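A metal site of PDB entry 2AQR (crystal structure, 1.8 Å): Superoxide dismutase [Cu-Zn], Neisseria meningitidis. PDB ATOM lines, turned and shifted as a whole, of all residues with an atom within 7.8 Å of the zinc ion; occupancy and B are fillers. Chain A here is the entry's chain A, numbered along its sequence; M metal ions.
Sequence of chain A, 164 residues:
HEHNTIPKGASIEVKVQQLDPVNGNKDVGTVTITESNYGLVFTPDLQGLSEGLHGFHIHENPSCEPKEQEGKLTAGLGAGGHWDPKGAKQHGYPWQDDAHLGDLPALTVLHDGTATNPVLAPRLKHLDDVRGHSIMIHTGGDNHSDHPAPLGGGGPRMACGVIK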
ATOM      1  N   PHE A  56     -26.085 -19.573  26.908  1.00  0.00           N
ATOM      2  CA  PHE A  56     -26.484 -19.018  28.196  1.00  0.00           C
ATOM      3  C   PHE A  56     -25.273 -18.301  28.798  1.00  0.00           C
ATOM      4  O   PHE A  56     -24.294 -18.954  29.162  1.00  0.00           O
ATOM      5  CB  PHE A  56     -26.936 -20.215  29.051  1.00  0.00           C
ATOM      6  CG  PHE A  56     -27.654 -19.863  30.321  1.00  0.00           C
ATOM      7  CD1 PHE A  56     -28.566 -18.814  30.369  1.00  0.00           C
ATOM      8  CD2 PHE A  56     -27.499 -20.679  31.442  1.00  0.00           C
ATOM      9  CE1 PHE A  56     -29.318 -18.583  31.526  1.00  0.00           C
ATOM     10  CE2 PHE A  56     -28.249 -20.461  32.593  1.00  0.00           C
ATOM     11  CZ  PHE A  56     -29.162 -19.412  32.641  1.00  0.00           C
ATOM     12  N   HIS A  57     -25.330 -16.977  28.881  1.00  0.00           N
ATOM     13  CA  HIS A  57     -24.187 -16.236  29.419  1.00  0.00           C
ATOM     14  C   HIS A  57     -24.554 -15.002  30.224  1.00  0.00           C
ATOM     15  O   HIS A  57     -25.654 -14.458  30.112  1.00  0.00           O
ATOM     16  CB  HIS A  57     -23.263 -15.747  28.301  1.00  0.00           C
ATOM     17  CG  HIS A  57     -23.309 -16.567  27.051  1.00  0.00           C
ATOM     18  ND1 HIS A  57     -23.967 -16.157  25.917  1.00  0.00           N
ATOM     19  CD2 HIS A  57     -22.752 -17.769  26.747  1.00  0.00           C
ATOM     20  CE1 HIS A  57     -23.824 -17.072  24.968  1.00  0.00           C
ATOM     21  NE2 HIS A  57     -23.082 -18.047  25.449  1.00  0.00           N
ATOM     22  N   ILE A  58     -23.600 -14.570  31.032  1.00  0.00           N
ATOM     23  CA  ILE A  58     -23.748 -13.350  31.810  1.00  0.00           C
ATOM     24  C   ILE A  58     -23.169 -12.265  30.910  1.00  0.00           C
ATOM     25  O   ILE A  58     -22.036 -12.395  30.435  1.00  0.00           O
ATOM     26  CB  ILE A  58     -22.896 -13.393  33.105  1.00  0.00           C
ATOM     27  CG1 ILE A  58     -23.332 -14.555  33.995  1.00  0.00           C
ATOM     28  CG2 ILE A  58     -23.019 -12.062  33.864  1.00  0.00           C
ATOM     29  CD1 ILE A  58     -24.764 -14.450  34.493  1.00  0.00           C
ATOM     30  N   HIS A  59     -23.943 -11.218  30.645  1.00  0.00           N
ATOM     31  CA  HIS A  59     -23.456 -10.118  29.831  1.00  0.00           C
ATOM     32  C   HIS A  59     -23.080  -8.945  30.727  1.00  0.00           C
ATOM     33  O   HIS A  59     -23.580  -8.825  31.841  1.00  0.00           O
ATOM     34  CB  HIS A  59     -24.490  -9.702  28.771  1.00  0.00           C
ATOM     35  CG  HIS A  59     -24.565 -10.658  27.623  1.00  0.00           C
ATOM     36  ND1 HIS A  59     -24.374 -10.270  26.323  1.00  0.00           N
ATOM     37  CD2 HIS A  59     -24.775 -11.992  27.593  1.00  0.00           C
ATOM     38  CE1 HIS A  59     -24.461 -11.323  25.531  1.00  0.00           C
ATOM     39  NE2 HIS A  59     -24.693 -12.388  26.282  1.00  0.00           N
ATOM     40  N   GLY A  81     -21.660  -7.010  25.593  1.00  0.00           N
ATOM     41  CA  GLY A  81     -21.120  -8.315  25.256  1.00  0.00           C
ATOM     42  C   GLY A  81     -21.003  -9.235  26.453  1.00  0.00           C
ATOM     43  O   GLY A  81     -21.500  -8.936  27.541  1.00  0.00           O
ATOM     44  N   HIS A  82     -20.348 -10.383  26.258  1.00  0.00           N
ATOM     45  CA  HIS A  82     -20.181 -11.323  27.348  1.00  0.00           C
ATOM     46  C   HIS A  82     -19.339 -10.694  28.454  1.00  0.00           C
ATOM     47  O   HIS A  82     -18.325 -10.036  28.175  1.00  0.00           O
ATOM     48  CB  HIS A  82     -19.491 -12.599  26.851  1.00  0.00           C
ATOM     49  CG  HIS A  82     -20.293 -13.384  25.863  1.00  0.00           C
ATOM     50  ND1 HIS A  82     -19.970 -14.671  25.504  1.00  0.00           N
ATOM     51  CD2 HIS A  82     -21.399 -13.062  25.151  1.00  0.00           C
ATOM     52  CE1 HIS A  82     -20.852 -15.111  24.623  1.00  0.00           C
ATOM     53  NE2 HIS A  82     -21.728 -14.155  24.397  1.00  0.00           N
ATOM     54  N   TRP A  83     -19.751 -10.881  29.694  1.00  0.00           N
ATOM     55  CA  TRP A  83     -19.013 -10.327  30.821  1.00  0.00           C
ATOM     56  C   TRP A  83     -17.610 -10.916  30.819  1.00  0.00           C
ATOM     57  O   TRP A  83     -17.429 -12.130  30.923  1.00  0.00           O
ATOM     58  CB  TRP A  83     -19.739 -10.631  32.137  1.00  0.00           C
ATOM     59  CG  TRP A  83     -19.138  -9.937  33.307  1.00  0.00           C
ATOM     60  CD1 TRP A  83     -18.711  -8.641  33.370  1.00  0.00           C
ATOM     61  CD2 TRP A  83     -18.894 -10.498  34.607  1.00  0.00           C
ATOM     62  NE1 TRP A  83     -18.223  -8.354  34.622  1.00  0.00           N
ATOM     63  CE2 TRP A  83     -18.333  -9.477  35.406  1.00  0.00           C
ATOM     64  CE3 TRP A  83     -19.113 -11.762  35.168  1.00  0.00           C
ATOM     65  CZ2 TRP A  83     -17.966  -9.684  36.742  1.00  0.00           C
ATOM     66  CZ3 TRP A  83     -18.759 -11.962  36.504  1.00  0.00           C
ATOM     67  CH2 TRP A  83     -18.192 -10.928  37.272  1.00  0.00           C
ATOM     68  N   ASP A  84     -16.620 -10.047  30.714  1.00  0.00           N
ATOM     69  CA  ASP A  84     -15.238 -10.474  30.643  1.00  0.00           C
ATOM     70  C   ASP A  84     -14.332  -9.569  31.482  1.00  0.00           C
ATOM     71  O   ASP A  84     -13.469  -8.871  30.955  1.00  0.00           O
ATOM     72  CB  ASP A  84     -14.819 -10.460  29.166  1.00  0.00           C
ATOM     73  CG  ASP A  84     -13.427 -11.010  28.926  1.00  0.00           C
ATOM     74  OD1 ASP A  84     -12.967 -11.853  29.712  1.00  0.00           O
ATOM     75  OD2 ASP A  84     -12.813 -10.594  27.929  1.00  0.00           O
ATOM     76  N   GLN A  90     -12.053 -13.959  24.706  1.00  0.00           N
ATOM     77  CA  GLN A  90     -12.253 -15.215  23.982  1.00  0.00           C
ATOM     78  C   GLN A  90     -13.423 -15.960  24.603  1.00  0.00           C
ATOM     79  O   GLN A  90     -13.551 -16.020  25.829  1.00  0.00           O
ATOM     80  CB  GLN A  90     -10.986 -16.058  24.091  1.00  0.00           C
ATOM     81  CG  GLN A  90     -11.052 -17.413  23.430  1.00  0.00           C
ATOM     82  CD  GLN A  90      -9.771 -18.214  23.629  1.00  0.00           C
ATOM     83  OE1 GLN A  90      -8.685 -17.738  23.312  1.00  0.00           O
ATOM     84  NE2 GLN A  90      -9.906 -19.429  24.155  1.00  0.00           N
ATOM     85  N   HIS A  91     -14.295 -16.518  23.769  1.00  0.00           N
ATOM     86  CA  HIS A  91     -15.436 -17.277  24.262  1.00  0.00           C
ATOM     87  C   HIS A  91     -14.994 -18.727  24.469  1.00  0.00           C
ATOM     88  O   HIS A  91     -14.285 -19.274  23.629  1.00  0.00           O
ATOM     89  CB  HIS A  91     -16.588 -17.228  23.276  1.00  0.00           C
ATOM     90  CG  HIS A  91     -17.820 -17.932  23.752  1.00  0.00           C
ATOM     91  ND1 HIS A  91     -18.574 -17.461  24.806  1.00  0.00           N
ATOM     92  CD2 HIS A  91     -18.383 -19.099  23.379  1.00  0.00           C
ATOM     93  CE1 HIS A  91     -19.546 -18.315  25.073  1.00  0.00           C
ATOM     94  NE2 HIS A  91     -19.449 -19.319  24.218  1.00  0.00           N
ATOM     95  N   GLY A  92     -15.404 -19.347  25.566  1.00  0.00           N
ATOM     96  CA  GLY A  92     -15.005 -20.723  25.802  1.00  0.00           C
ATOM     97  C   GLY A  92     -15.933 -21.515  26.697  1.00  0.00           C
ATOM     98  O   GLY A  92     -17.117 -21.219  26.797  1.00  0.00           O
ATOM     99  N   TYR A  93     -15.367 -22.527  27.348  1.00  0.00           N
ATOM    100  CA  TYR A  93     -16.125 -23.408  28.234  1.00  0.00           C
ATOM    101  C   TYR A  93     -16.301 -22.812  29.626  1.00  0.00           C
ATOM    102  O   TYR A  93     -15.535 -21.952  30.050  1.00  0.00           O
ATOM    103  CB  TYR A  93     -15.397 -24.753  28.367  1.00  0.00           C
ATOM    104  CG  TYR A  93     -15.387 -25.585  27.108  1.00  0.00           C
ATOM    105  CD1 TYR A  93     -16.495 -26.345  26.745  1.00  0.00           C
ATOM    106  CD2 TYR A  93     -14.282 -25.585  26.259  1.00  0.00           C
ATOM    107  CE1 TYR A  93     -16.502 -27.101  25.579  1.00  0.00           C
ATOM    108  CE2 TYR A  93     -14.284 -26.330  25.085  1.00  0.00           C
ATOM    109  CZ  TYR A  93     -15.394 -27.079  24.752  1.00  0.00           C
ATOM    110  OH  TYR A  93     -15.408 -27.813  23.587  1.00  0.00           O
ATOM    111  N   ALA A  99     -11.386 -17.994  29.293  1.00  0.00           N
ATOM    112  CA  ALA A  99     -12.594 -17.704  28.531  1.00  0.00           C
ATOM    113  C   ALA A  99     -13.368 -16.646  29.315  1.00  0.00           C
ATOM    114  O   ALA A  99     -13.099 -16.443  30.496  1.00  0.00           O
ATOM    115  CB  ALA A  99     -13.434 -18.962  28.371  1.00  0.00           C
ATOM    116  N   HIS A 100     -14.315 -15.976  28.667  1.00  0.00           N
ATOM    117  CA  HIS A 100     -15.135 -14.962  29.336  1.00  0.00           C
ATOM    118  C   HIS A 100     -15.649 -15.517  30.658  1.00  0.00           C
ATOM    119  O   HIS A 100     -16.119 -16.657  30.711  1.00  0.00           O
ATOM    120  CB  HIS A 100     -16.361 -14.605  28.497  1.00  0.00           C
ATOM    121  CG  HIS A 100     -16.048 -14.132  27.120  1.00  0.00           C
ATOM    122  ND1 HIS A 100     -16.765 -14.538  26.014  1.00  0.00           N
ATOM    123  CD2 HIS A 100     -15.138 -13.232  26.660  1.00  0.00           C
ATOM    124  CE1 HIS A 100     -16.327 -13.907  24.939  1.00  0.00           C
ATOM    125  NE2 HIS A 100     -15.340 -13.105  25.312  1.00  0.00           N
ATOM    126  N   LEU A 101     -15.569 -14.733  31.722  1.00  0.00           N
ATOM    127  CA  LEU A 101     -16.038 -15.205  33.024  1.00  0.00           C
ATOM    128  C   LEU A 101     -17.552 -15.422  32.993  1.00  0.00           C
ATOM    129  O   LEU A 101     -18.099 -16.158  33.816  1.00  0.00           O
ATOM    130  CB  LEU A 101     -15.686 -14.198  34.118  1.00  0.00           C
ATOM    131  CG  LEU A 101     -15.907 -14.662  35.559  1.00  0.00           C
ATOM    132  CD1 LEU A 101     -15.073 -15.902  35.829  1.00  0.00           C
ATOM    133  CD2 LEU A 101     -15.527 -13.554  36.523  1.00  0.00           C
ATOM    134  N   GLY A 102     -18.222 -14.793  32.037  1.00  0.00           N
ATOM    135  CA  GLY A 102     -19.664 -14.934  31.936  1.00  0.00           C
ATOM    136  C   GLY A 102     -20.159 -16.154  31.178  1.00  0.00           C
ATOM    137  O   GLY A 102     -21.367 -16.341  31.039  1.00  0.00           O
ATOM    138  N   ASP A 103     -19.241 -16.995  30.705  1.00  0.00           N
ATOM    139  CA  ASP A 103     -19.628 -18.181  29.935  1.00  0.00           C
ATOM    140  C   ASP A 103     -20.193 -19.303  30.815  1.00  0.00           C
ATOM    141  O   ASP A 103     -19.466 -19.934  31.582  1.00  0.00           O
ATOM    142  CB  ASP A 103     -18.444 -18.710  29.111  1.00  0.00           C
ATOM    143  CG  ASP A 103     -17.982 -17.722  28.050  1.00  0.00           C
ATOM    144  OD1 ASP A 103     -18.763 -16.805  27.703  1.00  0.00           O
ATOM    145  OD2 ASP A 103     -16.843 -17.854  27.562  1.00  0.00           O
ATOM    146  N   LEU A 104     -21.494 -19.526  30.696  1.00  0.00           N
ATOM    147  CA  LEU A 104     -22.172 -20.549  31.485  1.00  0.00           C
ATOM    148  C   LEU A 104     -22.501 -21.774  30.638  1.00  0.00           C
ATOM    149  O   LEU A 104     -22.413 -21.734  29.409  1.00  0.00           O
ATOM    150  CB  LEU A 104     -23.491 -19.979  32.044  1.00  0.00           C
ATOM    151  CG  LEU A 104     -23.468 -18.595  32.678  1.00  0.00           C
ATOM    152  CD1 LEU A 104     -24.909 -18.157  32.991  1.00  0.00           C
ATOM    153  CD2 LEU A 104     -22.628 -18.610  33.938  1.00  0.00           C
ATOM    154  N   ARG A 123     -16.440 -21.259  37.784  1.00  0.00           N
ATOM    155  CA  ARG A 123     -15.559 -20.112  37.910  1.00  0.00           C
ATOM    156  C   ARG A 123     -16.187 -18.937  38.641  1.00  0.00           C
ATOM    157  O   ARG A 123     -15.489 -18.022  39.077  1.00  0.00           O
ATOM    158  CB  ARG A 123     -15.067 -19.688  36.523  1.00  0.00           C
ATOM    159  CG  ARG A 123     -14.155 -20.740  35.885  1.00  0.00           C
ATOM    160  CD  ARG A 123     -13.520 -20.231  34.601  1.00  0.00           C
ATOM    161  NE  ARG A 123     -14.476 -20.171  33.499  1.00  0.00           N
ATOM    162  CZ  ARG A 123     -14.586 -19.152  32.654  1.00  0.00           C
ATOM    163  NH1 ARG A 123     -13.802 -18.083  32.788  1.00  0.00           N
ATOM    164  NH2 ARG A 123     -15.458 -19.205  31.670  1.00  0.00           N
ATOM    165  N   ASP A 142     -24.415 -23.225  21.797  1.00  0.00           N
ATOM    166  CA  ASP A 142     -23.120 -22.779  22.300  1.00  0.00           C
ATOM    167  C   ASP A 142     -22.103 -23.921  22.192  1.00  0.00           C
ATOM    168  O   ASP A 142     -22.194 -24.897  22.939  1.00  0.00           O
ATOM    169  CB  ASP A 142     -23.235 -22.326  23.763  1.00  0.00           C
ATOM    170  CG  ASP A 142     -22.048 -21.482  24.211  1.00  0.00           C
ATOM    171  OD1 ASP A 142     -20.992 -21.515  23.543  1.00  0.00           O
ATOM    172  OD2 ASP A 142     -22.162 -20.799  25.251  1.00  0.00           O
ATOM    173  N   HIS A 144     -19.080 -23.383  22.721  1.00  0.00           N
ATOM    174  CA  HIS A 144     -18.019 -22.856  23.580  1.00  0.00           C
ATOM    175  C   HIS A 144     -16.718 -22.520  22.872  1.00  0.00           C
ATOM    176  O   HIS A 144     -15.617 -22.806  23.359  1.00  0.00           O
ATOM    177  CB  HIS A 144     -17.767 -23.853  24.723  1.00  0.00           C
ATOM    178  CG  HIS A 144     -18.968 -24.066  25.595  1.00  0.00           C
ATOM    179  ND1 HIS A 144     -19.492 -23.091  26.404  1.00  0.00           N
ATOM    180  CD2 HIS A 144     -19.761 -25.151  25.749  1.00  0.00           C
ATOM    181  CE1 HIS A 144     -20.557 -23.554  27.022  1.00  0.00           C
ATOM    182  NE2 HIS A 144     -20.748 -24.807  26.642  1.00  0.00           N
ATOM    183  N   SER A 145     -16.847 -21.883  21.712  1.00  0.00           N
ATOM    184  CA  SER A 145     -15.696 -21.496  20.925  1.00  0.00           C
ATOM    185  C   SER A 145     -16.083 -20.331  20.006  1.00  0.00           C
ATOM    186  O   SER A 145     -17.263 -20.078  19.791  1.00  0.00           O
ATOM    187  CB  SER A 145     -15.224 -22.685  20.080  1.00  0.00           C
ATOM    188  OG  SER A 145     -14.104 -22.348  19.292  1.00  0.00           O
ATOM    189  N   ASP A 146     -15.080 -19.634  19.489  1.00  0.00           N
ATOM    190  CA  ASP A 146     -15.334 -18.518  18.585  1.00  0.00           C
ATOM    191  C   ASP A 146     -15.251 -18.991  17.141  1.00  0.00           C
ATOM    192  O   ASP A 146     -15.211 -18.185  16.206  1.00  0.00           O
ATOM    193  CB  ASP A 146     -14.358 -17.377  18.852  1.00  0.00           C
ATOM    194  CG  ASP A 146     -14.708 -16.592  20.098  1.00  0.00           C
ATOM    195  OD1 ASP A 146     -15.837 -16.070  20.168  1.00  0.00           O
ATOM    196  OD2 ASP A 146     -13.855 -16.492  21.015  1.00  0.00           O
ATOM    197  N   LEU A 151     -18.708 -16.228  19.443  1.00  0.00           N
ATOM    198  CA  LEU A 151     -19.475 -16.410  20.671  1.00  0.00           C
ATOM    199  C   LEU A 151     -20.292 -17.701  20.755  1.00  0.00           C
ATOM    200  O   LEU A 151     -21.441 -17.707  21.202  1.00  0.00           O
ATOM    201  CB  LEU A 151     -20.375 -15.189  20.869  1.00  0.00           C
ATOM    202  CG  LEU A 151     -19.605 -13.866  20.804  1.00  0.00           C
ATOM    203  CD1 LEU A 151     -20.573 -12.692  20.731  1.00  0.00           C
ATOM    204  CD2 LEU A 151     -18.686 -13.740  22.003  1.00  0.00           C
ATOM    205  N   GLY A 152     -19.676 -18.801  20.313  1.00  0.00           N
ATOM    206  CA  GLY A 152     -20.317 -20.113  20.373  1.00  0.00           C
ATOM    207  C   GLY A 152     -21.473 -20.365  19.430  1.00  0.00           C
ATOM    208  O   GLY A 152     -22.100 -21.422  19.491  1.00  0.00           O
HETATM  209 ZN    ZN M   1     -18.415 -15.828  26.074  1.00  0.00          ZN
HETATM  210 CU    CU M   2     -24.811 -14.269  25.575  1.00  0.00          CU
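The side-chain carboxylate of Asp 103 sits at hydrogen-bond distance from the backbone NH of Gly 92 (2.9 Å). A ring nitrogen (NE2) of His 82 sits close to a ring nitrogen (ND1) of His 57, 3.4 Å away. The side-chain carboxylate (OD1) of Asp 142 sits at hydrogen-bond distance from a ring nitrogen (NE2) of His 91 (2.8 Å). The side-chain carboxylate (OD2) of Asp 146 is in hydrogen-bond range of the backbone NH (N) of His 91, at 2.8 Å. The backbone NH (N) of His 100 is in hydrogen-bond range of the backbone carbonyl oxygen (O) of Gln 90 (2.9 Å). O of His 100 sits at hydrogen-bond distance from NH2 of Arg 123 (2.8 Å).
Four residues have an atom within 4 Å of the zinc ion: His 82, His 91, His 100 and Asp 103. Along chain A the residues within 4 Å of the zinc ion span positions 82 to 103.
The side-chain carboxylate (OD1) of Asp 103 is bound to the zinc ion (1.9 Å). A ring nitrogen (ND1) of His 82 is bound to the zinc ion, 2.0 Å away. The zinc ion is bound by ND1 of His 91, at 2.1 Å. The zinc ion is bound by ND1 of His 100.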
